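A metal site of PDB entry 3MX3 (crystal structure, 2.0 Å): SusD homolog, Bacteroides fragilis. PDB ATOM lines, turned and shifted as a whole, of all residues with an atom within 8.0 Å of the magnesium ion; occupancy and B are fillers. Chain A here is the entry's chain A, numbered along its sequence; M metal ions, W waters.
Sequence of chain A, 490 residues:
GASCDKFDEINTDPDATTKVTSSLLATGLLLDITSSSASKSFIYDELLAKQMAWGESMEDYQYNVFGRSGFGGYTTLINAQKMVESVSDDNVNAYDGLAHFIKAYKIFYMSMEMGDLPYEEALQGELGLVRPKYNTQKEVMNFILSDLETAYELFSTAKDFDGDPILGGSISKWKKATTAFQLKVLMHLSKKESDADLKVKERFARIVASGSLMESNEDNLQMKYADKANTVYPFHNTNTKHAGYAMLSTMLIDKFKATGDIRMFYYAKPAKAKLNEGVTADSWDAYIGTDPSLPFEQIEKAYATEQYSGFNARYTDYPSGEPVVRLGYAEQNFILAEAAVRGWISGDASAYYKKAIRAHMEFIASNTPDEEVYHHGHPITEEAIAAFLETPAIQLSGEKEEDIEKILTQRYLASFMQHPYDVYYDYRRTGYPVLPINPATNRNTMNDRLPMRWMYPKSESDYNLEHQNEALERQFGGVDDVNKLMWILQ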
ATOM      1  N   SER A  36       1.279 -26.730 -24.431  1.00  0.00           N
ATOM      2  CA  SER A  36       1.331 -25.266 -24.545  1.00  0.00           C
ATOM      3  C   SER A  36      -0.082 -24.713 -24.755  1.00  0.00           C
ATOM      4  O   SER A  36      -0.943 -25.411 -25.216  1.00  0.00           O
ATOM      5  CB  SER A  36       2.196 -24.859 -25.730  1.00  0.00           C
ATOM      6  OG  SER A  36       3.526 -25.344 -25.621  1.00  0.00           O
ATOM      7  N   SER A  39      -2.988 -19.888 -27.373  1.00  0.00           N
ATOM      8  CA  SER A  39      -3.399 -18.552 -27.093  1.00  0.00           C
ATOM      9  C   SER A  39      -2.181 -17.663 -26.938  1.00  0.00           C
ATOM     10  O   SER A  39      -1.022 -18.140 -26.914  1.00  0.00           O
ATOM     11  CB  SER A  39      -4.169 -18.507 -25.786  1.00  0.00           C
ATOM     12  OG  SER A  39      -3.287 -18.642 -24.683  1.00  0.00           O
ATOM     13  N   LYS A  40      -2.433 -16.381 -26.779  1.00  0.00           N
ATOM     14  CA  LYS A  40      -1.432 -15.343 -26.611  1.00  0.00           C
ATOM     15  C   LYS A  40      -0.365 -15.711 -25.585  1.00  0.00           C
ATOM     16  O   LYS A  40       0.802 -15.368 -25.713  1.00  0.00           O
ATOM     17  CB  LYS A  40      -2.131 -14.069 -26.153  1.00  0.00           C
ATOM     18  CG  LYS A  40      -1.523 -12.824 -26.651  1.00  0.00           C
ATOM     19  CD  LYS A  40      -1.855 -11.689 -25.691  1.00  0.00           C
ATOM     20  CE  LYS A  40      -3.216 -11.092 -25.956  1.00  0.00           C
ATOM     21  NZ  LYS A  40      -3.470 -10.020 -24.970  1.00  0.00           N
ATOM     22  N   SER A  41      -0.799 -16.375 -24.512  1.00  0.00           N
ATOM     23  CA  SER A  41       0.125 -16.747 -23.434  1.00  0.00           C
ATOM     24  C   SER A  41       1.359 -17.550 -23.887  1.00  0.00           C
ATOM     25  O   SER A  41       2.392 -17.506 -23.235  1.00  0.00           O
ATOM     26  CB  SER A  41      -0.577 -17.534 -22.343  1.00  0.00           C
ATOM     27  OG  SER A  41      -1.165 -18.710 -22.868  1.00  0.00           O
ATOM     28  N   PHE A  42       1.244 -18.289 -24.984  1.00  0.00           N
ATOM     29  CA  PHE A  42       2.361 -19.004 -25.645  1.00  0.00           C
ATOM     30  C   PHE A  42       3.584 -18.113 -25.878  1.00  0.00           C
ATOM     31  O   PHE A  42       4.734 -18.560 -25.773  1.00  0.00           O
ATOM     32  CB  PHE A  42       1.822 -19.561 -26.994  1.00  0.00           C
ATOM     33  CG  PHE A  42       2.715 -20.566 -27.671  1.00  0.00           C
ATOM     34  CD1 PHE A  42       3.251 -21.638 -26.981  1.00  0.00           C
ATOM     35  CD2 PHE A  42       2.990 -20.449 -29.038  1.00  0.00           C
ATOM     36  CE1 PHE A  42       4.054 -22.573 -27.621  1.00  0.00           C
ATOM     37  CE2 PHE A  42       3.799 -21.418 -29.689  1.00  0.00           C
ATOM     38  CZ  PHE A  42       4.309 -22.471 -28.972  1.00  0.00           C
ATOM     39  N   ILE A  43       3.336 -16.832 -26.163  1.00  0.00           N
ATOM     40  CA  ILE A  43       4.418 -15.918 -26.492  1.00  0.00           C
ATOM     41  C   ILE A  43       4.758 -14.921 -25.381  1.00  0.00           C
ATOM     42  O   ILE A  43       5.619 -14.049 -25.595  1.00  0.00           O
ATOM     43  CB  ILE A  43       4.183 -15.217 -27.887  1.00  0.00           C
ATOM     44  CG1 ILE A  43       2.832 -14.506 -27.967  1.00  0.00           C
ATOM     45  CG2 ILE A  43       4.308 -16.247 -29.015  1.00  0.00           C
ATOM     46  CD1 ILE A  43       2.699 -13.326 -27.039  1.00  0.00           C
ATOM     47  N   TYR A  44       4.113 -15.046 -24.215  1.00  0.00           N
ATOM     48  CA  TYR A  44       4.457 -14.225 -23.062  1.00  0.00           C
ATOM     49  C   TYR A  44       5.958 -14.302 -22.718  1.00  0.00           C
ATOM     50  O   TYR A  44       6.596 -13.289 -22.425  1.00  0.00           O
ATOM     51  CB  TYR A  44       3.624 -14.619 -21.851  1.00  0.00           C
ATOM     52  CG  TYR A  44       2.150 -14.158 -21.820  1.00  0.00           C
ATOM     53  CD1 TYR A  44       1.615 -13.247 -22.757  1.00  0.00           C
ATOM     54  CD2 TYR A  44       1.321 -14.608 -20.803  1.00  0.00           C
ATOM     55  CE1 TYR A  44       0.270 -12.832 -22.689  1.00  0.00           C
ATOM     56  CE2 TYR A  44       0.005 -14.200 -20.705  1.00  0.00           C
ATOM     57  CZ  TYR A  44      -0.522 -13.313 -21.655  1.00  0.00           C
ATOM     58  OH  TYR A  44      -1.826 -12.948 -21.514  1.00  0.00           O
ATOM     59  N   ASP A  45       6.532 -15.497 -22.761  1.00  0.00           N
ATOM     60  CA  ASP A  45       7.964 -15.649 -22.457  1.00  0.00           C
ATOM     61  C   ASP A  45       8.894 -15.069 -23.538  1.00  0.00           C
ATOM     62  O   ASP A  45       9.964 -14.571 -23.223  1.00  0.00           O
ATOM     63  CB  ASP A  45       8.326 -17.080 -22.101  1.00  0.00           C
ATOM     64  CG  ASP A  45       8.100 -18.073 -23.233  1.00  0.00           C
ATOM     65  OD1 ASP A  45       7.071 -18.047 -23.938  1.00  0.00           O
ATOM     66  OD2 ASP A  45       8.960 -18.950 -23.375  1.00  0.00           O
ATOM     67  N   GLU A  46       8.469 -15.134 -24.803  1.00  0.00           N
ATOM     68  CA  GLU A  46       9.147 -14.471 -25.907  1.00  0.00           C
ATOM     69  C   GLU A  46       9.074 -12.982 -25.708  1.00  0.00           C
ATOM     70  O   GLU A  46      10.044 -12.289 -25.928  1.00  0.00           O
ATOM     71  CB  GLU A  46       8.520 -14.816 -27.271  1.00  0.00           C
ATOM     72  CG  GLU A  46       9.042 -16.096 -27.967  1.00  0.00           C
ATOM     73  CD  GLU A  46       8.654 -17.358 -27.224  1.00  0.00           C
ATOM     74  OE1 GLU A  46       7.488 -17.416 -26.755  1.00  0.00           O
ATOM     75  OE2 GLU A  46       9.503 -18.278 -27.113  1.00  0.00           O
ATOM     76  N   LEU A  47       7.921 -12.465 -25.245  1.00  0.00           N
ATOM     77  CA  LEU A  47       7.816 -11.031 -24.943  1.00  0.00           C
ATOM     78  C   LEU A  47       8.723 -10.614 -23.762  1.00  0.00           C
ATOM     79  O   LEU A  47       9.385  -9.569 -23.807  1.00  0.00           O
ATOM     80  CB  LEU A  47       6.359 -10.634 -24.648  1.00  0.00           C
ATOM     81  CG  LEU A  47       5.306 -10.686 -25.744  1.00  0.00           C
ATOM     82  CD1 LEU A  47       3.935 -10.285 -25.168  1.00  0.00           C
ATOM     83  CD2 LEU A  47       5.682  -9.784 -26.930  1.00  0.00           C
ATOM     84  N   GLN A  51      12.184 -11.093 -27.582  1.00  0.00           N
ATOM     85  CA  GLN A  51      12.454 -11.719 -28.866  1.00  0.00           C
ATOM     86  C   GLN A  51      11.405 -11.300 -29.885  1.00  0.00           C
ATOM     87  O   GLN A  51      11.541 -11.532 -31.086  1.00  0.00           O
ATOM     88  CB  GLN A  51      12.458 -13.231 -28.707  1.00  0.00           C
ATOM     89  CG  GLN A  51      13.648 -13.736 -27.903  1.00  0.00           C
ATOM     90  CD  GLN A  51      13.658 -15.240 -27.755  1.00  0.00           C
ATOM     91  OE1 GLN A  51      12.609 -15.848 -27.603  1.00  0.00           O
ATOM     92  NE2 GLN A  51      14.854 -15.854 -27.812  1.00  0.00           N
ATOM     93  N   MET A  52      10.352 -10.674 -29.399  1.00  0.00           N
ATOM     94  CA  MET A  52       9.322 -10.104 -30.250  1.00  0.00           C
ATOM     95  C   MET A  52       8.493  -9.073 -29.523  1.00  0.00           C
ATOM     96  O   MET A  52       8.348  -9.117 -28.317  1.00  0.00           O
ATOM     97  CB  MET A  52       8.405 -11.209 -30.800  1.00  0.00           C
ATOM     98  CG  MET A  52       8.177 -12.394 -29.874  1.00  0.00           C
ATOM     99  SD  MET A  52       6.737 -13.557 -30.508  1.00  0.00           S
ATOM    100  CE  MET A  52       5.260 -12.648 -29.842  1.00  0.00           C
ATOM    101  N   TYR A 233       0.029 -27.387 -34.146  1.00  0.00           N
ATOM    102  CA  TYR A 233       0.936 -26.488 -33.424  1.00  0.00           C
ATOM    103  C   TYR A 233       0.108 -25.345 -32.787  1.00  0.00           C
ATOM    104  O   TYR A 233      -0.879 -24.863 -33.378  1.00  0.00           O
ATOM    105  CB  TYR A 233       2.008 -25.974 -34.408  1.00  0.00           C
ATOM    106  CG  TYR A 233       3.075 -25.084 -33.831  1.00  0.00           C
ATOM    107  CD1 TYR A 233       4.185 -25.614 -33.170  1.00  0.00           C
ATOM    108  CD2 TYR A 233       3.011 -23.728 -33.977  1.00  0.00           C
ATOM    109  CE1 TYR A 233       5.148 -24.809 -32.649  1.00  0.00           C
ATOM    110  CE2 TYR A 233       3.981 -22.892 -33.450  1.00  0.00           C
ATOM    111  CZ  TYR A 233       5.045 -23.442 -32.809  1.00  0.00           C
ATOM    112  OH  TYR A 233       5.990 -22.601 -32.320  1.00  0.00           O
ATOM    113  N   PHE A 235       0.066 -22.208 -32.544  1.00  0.00           N
ATOM    114  CA  PHE A 235      -0.204 -20.981 -33.333  1.00  0.00           C
ATOM    115  C   PHE A 235      -0.615 -21.234 -34.783  1.00  0.00           C
ATOM    116  O   PHE A 235      -0.634 -20.319 -35.601  1.00  0.00           O
ATOM    117  CB  PHE A 235       1.013 -20.049 -33.263  1.00  0.00           C
ATOM    118  CG  PHE A 235       0.921 -18.986 -32.197  1.00  0.00           C
ATOM    119  CD1 PHE A 235       0.051 -19.109 -31.120  1.00  0.00           C
ATOM    120  CD2 PHE A 235       1.728 -17.888 -32.259  1.00  0.00           C
ATOM    121  CE1 PHE A 235      -0.006 -18.114 -30.156  1.00  0.00           C
ATOM    122  CE2 PHE A 235       1.660 -16.904 -31.298  1.00  0.00           C
ATOM    123  CZ  PHE A 235       0.793 -17.022 -30.246  1.00  0.00           C
ATOM    124  N   VAL A 324       7.955 -28.474 -29.751  1.00  0.00           N
ATOM    125  CA  VAL A 324       8.213 -27.574 -28.610  1.00  0.00           C
ATOM    126  C   VAL A 324       8.991 -28.406 -27.621  1.00  0.00           C
ATOM    127  O   VAL A 324       8.483 -29.390 -27.025  1.00  0.00           O
ATOM    128  CB  VAL A 324       6.898 -27.006 -27.957  1.00  0.00           C
ATOM    129  CG1 VAL A 324       7.199 -26.239 -26.658  1.00  0.00           C
ATOM    130  CG2 VAL A 324       6.106 -26.124 -29.004  1.00  0.00           C
ATOM    131  N   SER A 415      16.502 -20.784 -29.005  1.00  0.00           N
ATOM    132  CA  SER A 415      15.424 -21.106 -28.080  1.00  0.00           C
ATOM    133  C   SER A 415      14.177 -20.220 -28.295  1.00  0.00           C
ATOM    134  O   SER A 415      13.283 -20.228 -27.490  1.00  0.00           O
ATOM    135  CB  SER A 415      15.922 -20.987 -26.637  1.00  0.00           C
ATOM    136  OG  SER A 415      15.014 -21.566 -25.721  1.00  0.00           O
ATOM    137  N   PHE A 416      14.160 -19.429 -29.383  1.00  0.00           N
ATOM    138  CA  PHE A 416      12.919 -18.738 -29.809  1.00  0.00           C
ATOM    139  C   PHE A 416      11.791 -19.747 -29.996  1.00  0.00           C
ATOM    140  O   PHE A 416      11.952 -20.700 -30.691  1.00  0.00           O
ATOM    141  CB  PHE A 416      13.189 -18.031 -31.127  1.00  0.00           C
ATOM    142  CG  PHE A 416      12.008 -17.253 -31.687  1.00  0.00           C
ATOM    143  CD1 PHE A 416      11.430 -16.234 -30.982  1.00  0.00           C
ATOM    144  CD2 PHE A 416      11.534 -17.515 -32.980  1.00  0.00           C
ATOM    145  CE1 PHE A 416      10.341 -15.512 -31.521  1.00  0.00           C
ATOM    146  CE2 PHE A 416      10.476 -16.796 -33.513  1.00  0.00           C
ATOM    147  CZ  PHE A 416       9.886 -15.800 -32.785  1.00  0.00           C
ATOM    148  N   MET A 417      10.649 -19.535 -29.333  1.00  0.00           N
ATOM    149  CA  MET A 417       9.505 -20.445 -29.369  1.00  0.00           C
ATOM    150  C   MET A 417       9.780 -21.827 -28.710  1.00  0.00           C
ATOM    151  O   MET A 417       9.045 -22.782 -28.932  1.00  0.00           O
ATOM    152  CB  MET A 417       8.896 -20.575 -30.775  1.00  0.00           C
ATOM    153  CG  MET A 417       8.605 -19.183 -31.447  1.00  0.00           C
ATOM    154  SD  MET A 417       7.128 -18.236 -30.616  1.00  0.00           S
ATOM    155  CE  MET A 417       5.723 -19.221 -31.529  1.00  0.00           C
ATOM    156  N   GLN A 418      10.795 -21.868 -27.854  1.00  0.00           N
ATOM    157  CA  GLN A 418      11.241 -23.100 -27.180  1.00  0.00           C
ATOM    158  C   GLN A 418      11.425 -22.895 -25.688  1.00  0.00           C
ATOM    159  O   GLN A 418      11.581 -21.761 -25.225  1.00  0.00           O
ATOM    160  CB  GLN A 418      12.578 -23.600 -27.794  1.00  0.00           C
ATOM    161  CG  GLN A 418      12.532 -23.916 -29.306  1.00  0.00           C
ATOM    162  CD  GLN A 418      11.591 -25.058 -29.623  1.00  0.00           C
ATOM    163  OE1 GLN A 418      11.272 -25.854 -28.754  1.00  0.00           O
ATOM    164  NE2 GLN A 418      11.146 -25.142 -30.893  1.00  0.00           N
ATOM    165  N   HIS A 419      11.433 -23.998 -24.926  1.00  0.00           N
ATOM    166  CA  HIS A 419      11.879 -23.988 -23.529  1.00  0.00           C
ATOM    167  C   HIS A 419      11.210 -22.874 -22.725  1.00  0.00           C
ATOM    168  O   HIS A 419      11.893 -21.919 -22.261  1.00  0.00           O
ATOM    169  CB  HIS A 419      13.399 -23.838 -23.441  1.00  0.00           C
ATOM    170  CG  HIS A 419      14.137 -24.925 -24.143  1.00  0.00           C
ATOM    171  ND1 HIS A 419      14.163 -26.233 -23.678  1.00  0.00           N
ATOM    172  CD2 HIS A 419      14.894 -24.914 -25.261  1.00  0.00           C
ATOM    173  CE1 HIS A 419      14.877 -26.964 -24.498  1.00  0.00           C
ATOM    174  NE2 HIS A 419      15.325 -26.196 -25.476  1.00  0.00           N
ATOM    175  N   PRO A 420       9.888 -23.005 -22.509  1.00  0.00           N
ATOM    176  CA  PRO A 420       9.151 -21.875 -21.935  1.00  0.00           C
ATOM    177  C   PRO A 420       9.812 -21.230 -20.686  1.00  0.00           C
ATOM    178  O   PRO A 420      10.095 -21.922 -19.716  1.00  0.00           O
ATOM    179  CB  PRO A 420       7.771 -22.486 -21.635  1.00  0.00           C
ATOM    180  CG  PRO A 420       7.607 -23.500 -22.692  1.00  0.00           C
ATOM    181  CD  PRO A 420       8.980 -24.129 -22.824  1.00  0.00           C
ATOM    182  N   TYR A 421      10.074 -19.918 -20.782  1.00  0.00           N
ATOM    183  CA  TYR A 421      10.694 -19.074 -19.719  1.00  0.00           C
ATOM    184  C   TYR A 421      12.173 -19.298 -19.392  1.00  0.00           C
ATOM    185  O   TYR A 421      12.759 -18.508 -18.661  1.00  0.00           O
ATOM    186  CB  TYR A 421       9.847 -18.977 -18.399  1.00  0.00           C
ATOM    187  CG  TYR A 421       8.469 -18.331 -18.593  1.00  0.00           C
ATOM    188  CD1 TYR A 421       8.296 -16.965 -18.520  1.00  0.00           C
ATOM    189  CD2 TYR A 421       7.347 -19.122 -18.947  1.00  0.00           C
ATOM    190  CE1 TYR A 421       7.075 -16.379 -18.728  1.00  0.00           C
ATOM    191  CE2 TYR A 421       6.102 -18.523 -19.195  1.00  0.00           C
ATOM    192  CZ  TYR A 421       6.004 -17.157 -19.093  1.00  0.00           C
ATOM    193  OH  TYR A 421       4.792 -16.562 -19.298  1.00  0.00           O
HETATM  194 MG    MG M   1       6.711 -19.092 -25.659  1.00  0.00          MG
HETATM  195  O   HOH W   1       8.478 -20.130 -25.514  1.00  0.00           O
HETATM  196  O   HOH W   2       5.985 -20.857 -24.568  1.00  0.00           O
HETATM  197  O   HOH W   3       6.362 -20.227 -27.501  1.00  0.00           O
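The backbone NH (N) of Met 417 lies within hydrogen-bond range of the side-chain carboxylate (OE2) of Glu 46, at 2.8 Å. OD2 of Asp 45 lies within hydrogen-bond range of N of Tyr 421 (3.0 Å). The backbone carbonyl oxygen of Glu 46 lies within hydrogen-bond range of the backbone NH of Gln 51 (3.0 Å).
Of the 22 residues printed, 3 come within 4 Å of the magnesium ion. The nearest printed residue that does not touch the magnesium ion is Ile 43 (4.003 Å).
The magnesium ion is bound by OD1 of Asp 45, O of Phe 42, water W1, OE1 of Glu 46, water W3 and water W2.
Water W1 bridges OD2 of Asp 45 and OE2 of Glu 46.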
